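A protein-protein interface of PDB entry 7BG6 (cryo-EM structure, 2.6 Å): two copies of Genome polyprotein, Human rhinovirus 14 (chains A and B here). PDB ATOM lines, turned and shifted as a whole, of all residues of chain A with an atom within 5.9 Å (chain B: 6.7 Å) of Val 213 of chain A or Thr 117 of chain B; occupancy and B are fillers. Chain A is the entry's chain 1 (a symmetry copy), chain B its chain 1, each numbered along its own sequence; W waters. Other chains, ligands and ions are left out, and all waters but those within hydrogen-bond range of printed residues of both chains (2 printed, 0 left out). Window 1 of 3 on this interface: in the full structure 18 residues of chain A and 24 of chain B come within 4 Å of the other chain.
The side-chain amide nitrogen of Asn 214 of chain A lies within hydrogen-bond range of the backbone carbonyl oxygen of Ala 118 of chain B (3.1 Å).
The side-chain amino group of Lys 224 of chain B lies within salt-bridge range of the side-chain carboxylate of Glu 215 of chain A, 2.8 Å away.
OD1 of Asn 214 of chain A sits at hydrogen-bond distance from N of Val 131 of chain A (2.7 Å).
The side-chain amide oxygen (OE1) of Gln 133 of chain A sits at hydrogen-bond distance from the guanidinium group (NE) of Arg 211 of chain A, 2.7 Å away.
The backbone carbonyl oxygen (O) of Ser 119 of chain B is in hydrogen-bond range of the backbone NH (N) of Leu 222 of chain B (2.7 Å).
O of Val 131 of chain A lies within hydrogen-bond range of N of Val 213 of chain A (2.9 Å).
The backbone carbonyl oxygen (O) of Thr 117 of chain B is in hydrogen-bond range of the backbone NH (N) of Lys 224 of chain B (3.0 Å).
ND2 of Asn 214 of chain A sits at hydrogen-bond distance from O of Asn 129 of chain A (3.3 Å).
Thr 117 of chain B touches Val 131 of chain A (CG2 to CG2, 3.8 Å).
Gly 165 of chain B touches Val 131 of chain A.
CD2 of Phe 161 of chain A touches CD2 of Leu 115 of chain B, 3.6 Å away.
Phe 161 of chain A touches Tyr 228 of chain B.
Arg 226 of chain B touches Arg 211 of chain A.
CG2 of Val 213 of chain A touches CG2 of Thr 117 of chain B (3.7 Å).
Asn 214 of chain A touches Thr 117 of chain B (OD1 to CG2, 3.6 Å).
CB of Glu 215 of chain A touches OG of Ser 119 of chain B, 3.3 Å away.
Of the printed residues of chain B, Val 131 of chain A touches Thr 117 (3.8 Å) and Gly 165 (3.6 Å).
Of the printed residues of chain A, Ala 118 of chain B touches Asn 214 (3.1 Å).
Val 223 of chain B touches none of the printed residues of chain A.
The nearest residue of chain B that does not touch Val 213 of chain A is Arg 226 of chain B (4.1 Å).
The nearest printed residue of chain B that does not touch Glu 215 of chain A is Ala 118 of chain B (4.7 Å).
Printed residues of chain A that touch a printed residue of chain B: Val 131, Phe 161, Arg 211, Val 213, Asn 214 and Glu 215.
Among the printed residues, 10 pairs touch across the chains.
Among the printed residues, Asp or Glu carboxylates within 4 Å of a Lys or Arg side-chain nitrogen of the other chain: Glu 215 of chain A with Lys 224 of chain B (2.8 Å).
No position is printed for both chains.
Of the 10 pairs that touch across the chains among the printed residues, none has its exchanged pair printed and touching as well.
Water W2 bridges the backbone carbonyl oxygen (O) of Thr 117 of chain B (2.6 Å) and the backbone NH (N) of Glu 215 of chain A (3.1 Å).
Water W1 lies within hydrogen-bond range of the backbone NH of Ala 118 of chain B, the backbone carbonyl oxygen of Asn 129 of chain A and the side-chain amide nitrogen of Asn 214 of chain A.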
ATOM      1  N   ASN A 129      -6.497  11.970  -0.504  1.00  0.00           N
ATOM      2  CA  ASN A 129      -7.927  12.079  -0.736  1.00  0.00           C
ATOM      3  C   ASN A 129      -8.274  13.542  -1.002  1.00  0.00           C
ATOM      4  O   ASN A 129      -8.924  14.199  -0.189  1.00  0.00           O
ATOM      5  CB  ASN A 129      -8.730  11.398   0.376  1.00  0.00           C
ATOM      6  CG  ASN A 129      -8.561   9.894   0.370  1.00  0.00           C
ATOM      7  OD1 ASN A 129      -9.152   9.201  -0.456  1.00  0.00           O
ATOM      8  ND2 ASN A 129      -7.754   9.379   1.284  1.00  0.00           N
ATOM      9  N   LEU A 130      -7.825  14.022  -2.165  1.00  0.00           N
ATOM     10  CA  LEU A 130      -7.914  15.419  -2.553  1.00  0.00           C
ATOM     11  C   LEU A 130      -9.345  15.750  -2.961  1.00  0.00           C
ATOM     12  O   LEU A 130     -10.050  14.911  -3.520  1.00  0.00           O
ATOM     13  CB  LEU A 130      -6.955  15.671  -3.723  1.00  0.00           C
ATOM     14  CG  LEU A 130      -5.541  15.114  -3.569  1.00  0.00           C
ATOM     15  CD1 LEU A 130      -4.825  15.084  -4.908  1.00  0.00           C
ATOM     16  CD2 LEU A 130      -4.744  15.919  -2.555  1.00  0.00           C
ATOM     17  N   VAL A 131      -9.751  16.990  -2.670  1.00  0.00           N
ATOM     18  CA  VAL A 131     -11.019  17.531  -3.128  1.00  0.00           C
ATOM     19  C   VAL A 131     -10.721  18.694  -4.070  1.00  0.00           C
ATOM     20  O   VAL A 131     -10.064  19.661  -3.685  1.00  0.00           O
ATOM     21  CB  VAL A 131     -11.919  17.951  -1.947  1.00  0.00           C
ATOM     22  CG1 VAL A 131     -13.107  18.792  -2.397  1.00  0.00           C
ATOM     23  CG2 VAL A 131     -12.394  16.750  -1.142  1.00  0.00           C
ATOM     24  N   VAL A 132     -11.192  18.567  -5.316  1.00  0.00           N
ATOM     25  CA  VAL A 132     -11.052  19.617  -6.312  1.00  0.00           C
ATOM     26  C   VAL A 132     -12.243  20.562  -6.191  1.00  0.00           C
ATOM     27  O   VAL A 132     -13.373  20.117  -5.990  1.00  0.00           O
ATOM     28  CB  VAL A 132     -10.927  19.039  -7.737  1.00  0.00           C
ATOM     29  CG1 VAL A 132     -11.221  20.074  -8.814  1.00  0.00           C
ATOM     30  CG2 VAL A 132      -9.565  18.407  -7.975  1.00  0.00           C
ATOM     31  N   GLN A 133     -11.968  21.866  -6.297  1.00  0.00           N
ATOM     32  CA  GLN A 133     -13.016  22.857  -6.467  1.00  0.00           C
ATOM     33  C   GLN A 133     -13.020  23.335  -7.916  1.00  0.00           C
ATOM     34  O   GLN A 133     -12.014  23.839  -8.412  1.00  0.00           O
ATOM     35  CB  GLN A 133     -12.845  24.036  -5.507  1.00  0.00           C
ATOM     36  CG  GLN A 133     -13.924  25.099  -5.673  1.00  0.00           C
ATOM     37  CD  GLN A 133     -13.761  26.297  -4.770  1.00  0.00           C
ATOM     38  OE1 GLN A 133     -12.740  26.475  -4.110  1.00  0.00           O
ATOM     39  NE2 GLN A 133     -14.780  27.140  -4.735  1.00  0.00           N
ATOM     40  N   TRP A 147      -4.467  30.417  -4.892  1.00  0.00           N
ATOM     41  CA  TRP A 147      -5.176  29.150  -4.797  1.00  0.00           C
ATOM     42  C   TRP A 147      -6.164  29.152  -3.629  1.00  0.00           C
ATOM     43  O   TRP A 147      -7.105  28.365  -3.624  1.00  0.00           O
ATOM     44  CB  TRP A 147      -4.202  27.963  -4.744  1.00  0.00           C
ATOM     45  CG  TRP A 147      -3.658  27.666  -3.379  1.00  0.00           C
ATOM     46  CD1 TRP A 147      -2.486  28.116  -2.846  1.00  0.00           C
ATOM     47  CD2 TRP A 147      -4.269  26.845  -2.367  1.00  0.00           C
ATOM     48  NE1 TRP A 147      -2.326  27.638  -1.574  1.00  0.00           N
ATOM     49  CE2 TRP A 147      -3.402  26.855  -1.252  1.00  0.00           C
ATOM     50  CE3 TRP A 147      -5.457  26.107  -2.290  1.00  0.00           C
ATOM     51  CZ2 TRP A 147      -3.691  26.156  -0.080  1.00  0.00           C
ATOM     52  CZ3 TRP A 147      -5.742  25.419  -1.130  1.00  0.00           C
ATOM     53  CH2 TRP A 147      -4.869  25.443  -0.041  1.00  0.00           C
ATOM     54  N   PHE A 161     -17.470  21.073  -5.441  1.00  0.00           N
ATOM     55  CA  PHE A 161     -16.417  20.350  -4.749  1.00  0.00           C
ATOM     56  C   PHE A 161     -16.660  18.854  -4.918  1.00  0.00           C
ATOM     57  O   PHE A 161     -17.765  18.372  -4.678  1.00  0.00           O
ATOM     58  CB  PHE A 161     -16.381  20.722  -3.264  1.00  0.00           C
ATOM     59  CG  PHE A 161     -16.203  22.192  -2.983  1.00  0.00           C
ATOM     60  CD1 PHE A 161     -17.280  23.064  -3.070  1.00  0.00           C
ATOM     61  CD2 PHE A 161     -14.964  22.704  -2.634  1.00  0.00           C
ATOM     62  CE1 PHE A 161     -17.120  24.417  -2.813  1.00  0.00           C
ATOM     63  CE2 PHE A 161     -14.807  24.057  -2.371  1.00  0.00           C
ATOM     64  CZ  PHE A 161     -15.883  24.911  -2.468  1.00  0.00           C
ATOM     65  N   ARG A 211      -8.982  24.192  -8.573  1.00  0.00           N
ATOM     66  CA  ARG A 211      -7.972  24.080  -7.535  1.00  0.00           C
ATOM     67  C   ARG A 211      -8.241  22.821  -6.717  1.00  0.00           C
ATOM     68  O   ARG A 211      -9.338  22.271  -6.760  1.00  0.00           O
ATOM     69  CB  ARG A 211      -7.985  25.320  -6.633  1.00  0.00           C
ATOM     70  CG  ARG A 211      -9.208  25.428  -5.733  1.00  0.00           C
ATOM     71  CD  ARG A 211      -8.940  26.288  -4.513  1.00  0.00           C
ATOM     72  NE  ARG A 211     -10.109  26.453  -3.661  1.00  0.00           N
ATOM     73  CZ  ARG A 211     -10.103  27.026  -2.459  1.00  0.00           C
ATOM     74  NH1 ARG A 211      -8.979  27.497  -1.949  1.00  0.00           N
ATOM     75  NH2 ARG A 211     -11.226  27.124  -1.771  1.00  0.00           N
ATOM     76  N   ILE A 212      -7.217  22.375  -5.983  1.00  0.00           N
ATOM     77  CA  ILE A 212      -7.381  21.360  -4.956  1.00  0.00           C
ATOM     78  C   ILE A 212      -7.403  22.077  -3.609  1.00  0.00           C
ATOM     79  O   ILE A 212      -6.428  22.726  -3.233  1.00  0.00           O
ATOM     80  CB  ILE A 212      -6.269  20.295  -5.052  1.00  0.00           C
ATOM     81  CG1 ILE A 212      -6.340  19.533  -6.379  1.00  0.00           C
ATOM     82  CG2 ILE A 212      -6.322  19.348  -3.860  1.00  0.00           C
ATOM     83  CD1 ILE A 212      -4.993  19.169  -6.958  1.00  0.00           C
ATOM     84  N   VAL A 213      -8.536  21.960  -2.903  1.00  0.00           N
ATOM     85  CA  VAL A 213      -8.795  22.737  -1.699  1.00  0.00           C
ATOM     86  C   VAL A 213      -7.934  22.223  -0.548  1.00  0.00           C
ATOM     87  O   VAL A 213      -7.739  22.930   0.441  1.00  0.00           O
ATOM     88  CB  VAL A 213     -10.291  22.761  -1.321  1.00  0.00           C
ATOM     89  CG1 VAL A 213     -11.147  23.398  -2.403  1.00  0.00           C
ATOM     90  CG2 VAL A 213     -10.824  21.385  -0.949  1.00  0.00           C
ATOM     91  N   ASN A 214      -7.434  20.989  -0.686  1.00  0.00           N
ATOM     92  CA  ASN A 214      -6.582  20.379   0.321  1.00  0.00           C
ATOM     93  C   ASN A 214      -5.293  21.180   0.448  1.00  0.00           C
ATOM     94  O   ASN A 214      -4.780  21.710  -0.537  1.00  0.00           O
ATOM     95  CB  ASN A 214      -6.246  18.924  -0.015  1.00  0.00           C
ATOM     96  CG  ASN A 214      -7.452  18.009   0.002  1.00  0.00           C
ATOM     97  OD1 ASN A 214      -8.441  18.267  -0.680  1.00  0.00           O
ATOM     98  ND2 ASN A 214      -7.375  16.934   0.767  1.00  0.00           N
ATOM     99  N   GLU A 215      -4.784  21.261   1.683  1.00  0.00           N
ATOM    100  CA  GLU A 215      -3.427  21.716   1.921  1.00  0.00           C
ATOM    101  C   GLU A 215      -2.471  20.676   1.343  1.00  0.00           C
ATOM    102  O   GLU A 215      -2.898  19.624   0.868  1.00  0.00           O
ATOM    103  CB  GLU A 215      -3.188  21.957   3.413  1.00  0.00           C
ATOM    104  CG  GLU A 215      -4.036  23.073   4.002  1.00  0.00           C
ATOM    105  CD  GLU A 215      -3.770  24.470   3.459  1.00  0.00           C
ATOM    106  OE1 GLU A 215      -2.599  24.776   3.153  1.00  0.00           O
ATOM    107  OE2 GLU A 215      -4.736  25.246   3.339  1.00  0.00           O
ATOM    108  N   LEU B 115     -17.082  21.004   5.014  1.00  0.00           N
ATOM    109  CA  LEU B 115     -16.162  20.217   4.210  1.00  0.00           C
ATOM    110  C   LEU B 115     -14.805  20.163   4.907  1.00  0.00           C
ATOM    111  O   LEU B 115     -14.121  21.178   5.033  1.00  0.00           O
ATOM    112  CB  LEU B 115     -16.066  20.839   2.810  1.00  0.00           C
ATOM    113  CG  LEU B 115     -14.927  20.344   1.917  1.00  0.00           C
ATOM    114  CD1 LEU B 115     -15.097  18.876   1.549  1.00  0.00           C
ATOM    115  CD2 LEU B 115     -14.819  21.192   0.660  1.00  0.00           C
ATOM    116  N   ALA B 116     -14.440  18.960   5.364  1.00  0.00           N
ATOM    117  CA  ALA B 116     -13.153  18.717   5.993  1.00  0.00           C
ATOM    118  C   ALA B 116     -12.222  18.039   4.994  1.00  0.00           C
ATOM    119  O   ALA B 116     -12.587  17.041   4.377  1.00  0.00           O
ATOM    120  CB  ALA B 116     -13.334  17.884   7.238  1.00  0.00           C
ATOM    121  N   THR B 117     -11.022  18.611   4.836  1.00  0.00           N
ATOM    122  CA  THR B 117     -10.000  18.073   3.954  1.00  0.00           C
ATOM    123  C   THR B 117      -8.693  17.939   4.729  1.00  0.00           C
ATOM    124  O   THR B 117      -8.284  18.866   5.427  1.00  0.00           O
ATOM    125  CB  THR B 117      -9.842  18.929   2.689  1.00  0.00           C
ATOM    126  OG1 THR B 117      -9.689  20.293   3.081  1.00  0.00           O
ATOM    127  CG2 THR B 117     -11.010  18.798   1.735  1.00  0.00           C
ATOM    128  N   ALA B 118      -8.051  16.773   4.593  1.00  0.00           N
ATOM    129  CA  ALA B 118      -6.868  16.439   5.370  1.00  0.00           C
ATOM    130  C   ALA B 118      -5.603  16.692   4.556  1.00  0.00           C
ATOM    131  O   ALA B 118      -5.636  16.714   3.326  1.00  0.00           O
ATOM    132  CB  ALA B 118      -6.941  15.004   5.831  1.00  0.00           C
ATOM    133  N   SER B 119      -4.494  16.880   5.278  1.00  0.00           N
ATOM    134  CA  SER B 119      -3.165  16.989   4.700  1.00  0.00           C
ATOM    135  C   SER B 119      -2.136  16.510   5.720  1.00  0.00           C
ATOM    136  O   SER B 119      -2.214  16.859   6.896  1.00  0.00           O
ATOM    137  CB  SER B 119      -2.880  18.400   4.256  1.00  0.00           C
ATOM    138  OG  SER B 119      -2.837  19.282   5.368  1.00  0.00           O
ATOM    139  N   VAL B 164     -13.470  12.785   7.111  1.00  0.00           N
ATOM    140  CA  VAL B 164     -12.637  13.801   6.487  1.00  0.00           C
ATOM    141  C   VAL B 164     -12.462  13.436   5.015  1.00  0.00           C
ATOM    142  O   VAL B 164     -12.216  12.278   4.682  1.00  0.00           O
ATOM    143  CB  VAL B 164     -11.283  13.946   7.210  1.00  0.00           C
ATOM    144  CG1 VAL B 164     -10.351  14.908   6.490  1.00  0.00           C
ATOM    145  CG2 VAL B 164     -11.459  14.372   8.658  1.00  0.00           C
ATOM    146  N   GLY B 165     -12.592  14.445   4.147  1.00  0.00           N
ATOM    147  CA  GLY B 165     -12.661  14.238   2.710  1.00  0.00           C
ATOM    148  C   GLY B 165     -14.108  14.297   2.230  1.00  0.00           C
ATOM    149  O   GLY B 165     -14.388  14.797   1.142  1.00  0.00           O
ATOM    150  N   ASP B 166     -15.012  13.774   3.067  1.00  0.00           N
ATOM    151  CA  ASP B 166     -16.445  13.853   2.838  1.00  0.00           C
ATOM    152  C   ASP B 166     -16.996  15.094   3.533  1.00  0.00           C
ATOM    153  O   ASP B 166     -16.235  15.908   4.057  1.00  0.00           O
ATOM    154  CB  ASP B 166     -17.150  12.556   3.250  1.00  0.00           C
ATOM    155  CG  ASP B 166     -16.869  11.386   2.322  1.00  0.00           C
ATOM    156  OD1 ASP B 166     -16.256  11.610   1.259  1.00  0.00           O
ATOM    157  OD2 ASP B 166     -17.265  10.257   2.670  1.00  0.00           O
ATOM    158  N   LEU B 222      -3.161  17.417   9.349  1.00  0.00           N
ATOM    159  CA  LEU B 222      -3.781  18.724   9.487  1.00  0.00           C
ATOM    160  C   LEU B 222      -5.090  18.724   8.703  1.00  0.00           C
ATOM    161  O   LEU B 222      -5.097  18.447   7.505  1.00  0.00           O
ATOM    162  CB  LEU B 222      -2.813  19.784   8.949  1.00  0.00           C
ATOM    163  CG  LEU B 222      -1.638  20.169   9.852  1.00  0.00           C
ATOM    164  CD1 LEU B 222      -0.786  18.963  10.224  1.00  0.00           C
ATOM    165  CD2 LEU B 222      -0.773  21.225   9.180  1.00  0.00           C
ATOM    166  N   VAL B 223      -6.193  19.023   9.397  1.00  0.00           N
ATOM    167  CA  VAL B 223      -7.509  19.027   8.780  1.00  0.00           C
ATOM    168  C   VAL B 223      -8.033  20.460   8.735  1.00  0.00           C
ATOM    169  O   VAL B 223      -8.329  21.057   9.770  1.00  0.00           O
ATOM    170  CB  VAL B 223      -8.488  18.070   9.493  1.00  0.00           C
ATOM    171  CG1 VAL B 223      -9.894  18.157   8.915  1.00  0.00           C
ATOM    172  CG2 VAL B 223      -7.992  16.633   9.456  1.00  0.00           C
ATOM    173  N   LYS B 224      -8.126  20.995   7.514  1.00  0.00           N
ATOM    174  CA  LYS B 224      -8.713  22.302   7.276  1.00  0.00           C
ATOM    175  C   LYS B 224     -10.210  22.126   7.035  1.00  0.00           C
ATOM    176  O   LYS B 224     -10.619  21.498   6.059  1.00  0.00           O
ATOM    177  CB  LYS B 224      -8.010  22.999   6.107  1.00  0.00           C
ATOM    178  CG  LYS B 224      -8.492  24.413   5.808  1.00  0.00           C
ATOM    179  CD  LYS B 224      -7.426  25.309   5.212  1.00  0.00           C
ATOM    180  CE  LYS B 224      -6.445  25.831   6.239  1.00  0.00           C
ATOM    181  NZ  LYS B 224      -5.432  26.725   5.627  1.00  0.00           N
ATOM    182  N   ILE B 225     -11.011  22.676   7.953  1.00  0.00           N
ATOM    183  CA  ILE B 225     -12.460  22.597   7.882  1.00  0.00           C
ATOM    184  C   ILE B 225     -12.988  23.897   7.280  1.00  0.00           C
ATOM    185  O   ILE B 225     -12.568  24.983   7.677  1.00  0.00           O
ATOM    186  CB  ILE B 225     -13.058  22.301   9.274  1.00  0.00           C
ATOM    187  CG1 ILE B 225     -12.721  20.880   9.734  1.00  0.00           C
ATOM    188  CG2 ILE B 225     -14.557  22.561   9.298  1.00  0.00           C
ATOM    189  CD1 ILE B 225     -13.005  20.613  11.193  1.00  0.00           C
ATOM    190  N   ARG B 226     -13.900  23.760   6.312  1.00  0.00           N
ATOM    191  CA  ARG B 226     -14.525  24.894   5.652  1.00  0.00           C
ATOM    192  C   ARG B 226     -16.036  24.814   5.846  1.00  0.00           C
ATOM    193  O   ARG B 226     -16.672  23.854   5.411  1.00  0.00           O
ATOM    194  CB  ARG B 226     -14.167  24.913   4.161  1.00  0.00           C
ATOM    195  CG  ARG B 226     -12.686  25.112   3.873  1.00  0.00           C
ATOM    196  CD  ARG B 226     -12.394  25.115   2.385  1.00  0.00           C
ATOM    197  NE  ARG B 226     -10.982  25.332   2.097  1.00  0.00           N
ATOM    198  CZ  ARG B 226     -10.407  26.523   1.960  1.00  0.00           C
ATOM    199  NH1 ARG B 226     -11.119  27.629   2.087  1.00  0.00           N
ATOM    200  NH2 ARG B 226      -9.114  26.602   1.697  1.00  0.00           N
ATOM    201  N   TYR B 228     -19.711  26.148   5.030  1.00  0.00           N
ATOM    202  CA  TYR B 228     -20.481  26.810   3.991  1.00  0.00           C
ATOM    203  C   TYR B 228     -21.907  27.031   4.486  1.00  0.00           C
ATOM    204  O   TYR B 228     -22.509  26.135   5.071  1.00  0.00           O
ATOM    205  CB  TYR B 228     -20.444  26.003   2.689  1.00  0.00           C
ATOM    206  CG  TYR B 228     -19.139  26.104   1.942  1.00  0.00           C
ATOM    207  CD1 TYR B 228     -18.027  25.381   2.346  1.00  0.00           C
ATOM    208  CD2 TYR B 228     -19.010  26.933   0.838  1.00  0.00           C
ATOM    209  CE1 TYR B 228     -16.820  25.476   1.672  1.00  0.00           C
ATOM    210  CE2 TYR B 228     -17.810  27.037   0.151  1.00  0.00           C
ATOM    211  CZ  TYR B 228     -16.712  26.306   0.570  1.00  0.00           C
ATOM    212  OH  TYR B 228     -15.524  26.404  -0.094  1.00  0.00           O
HETATM  213  O   HOH W   1      -8.927  15.064   2.675  1.00  0.00           O
HETATM  214  O   HOH W   2      -6.824  20.236   3.789  1.00  0.00           O
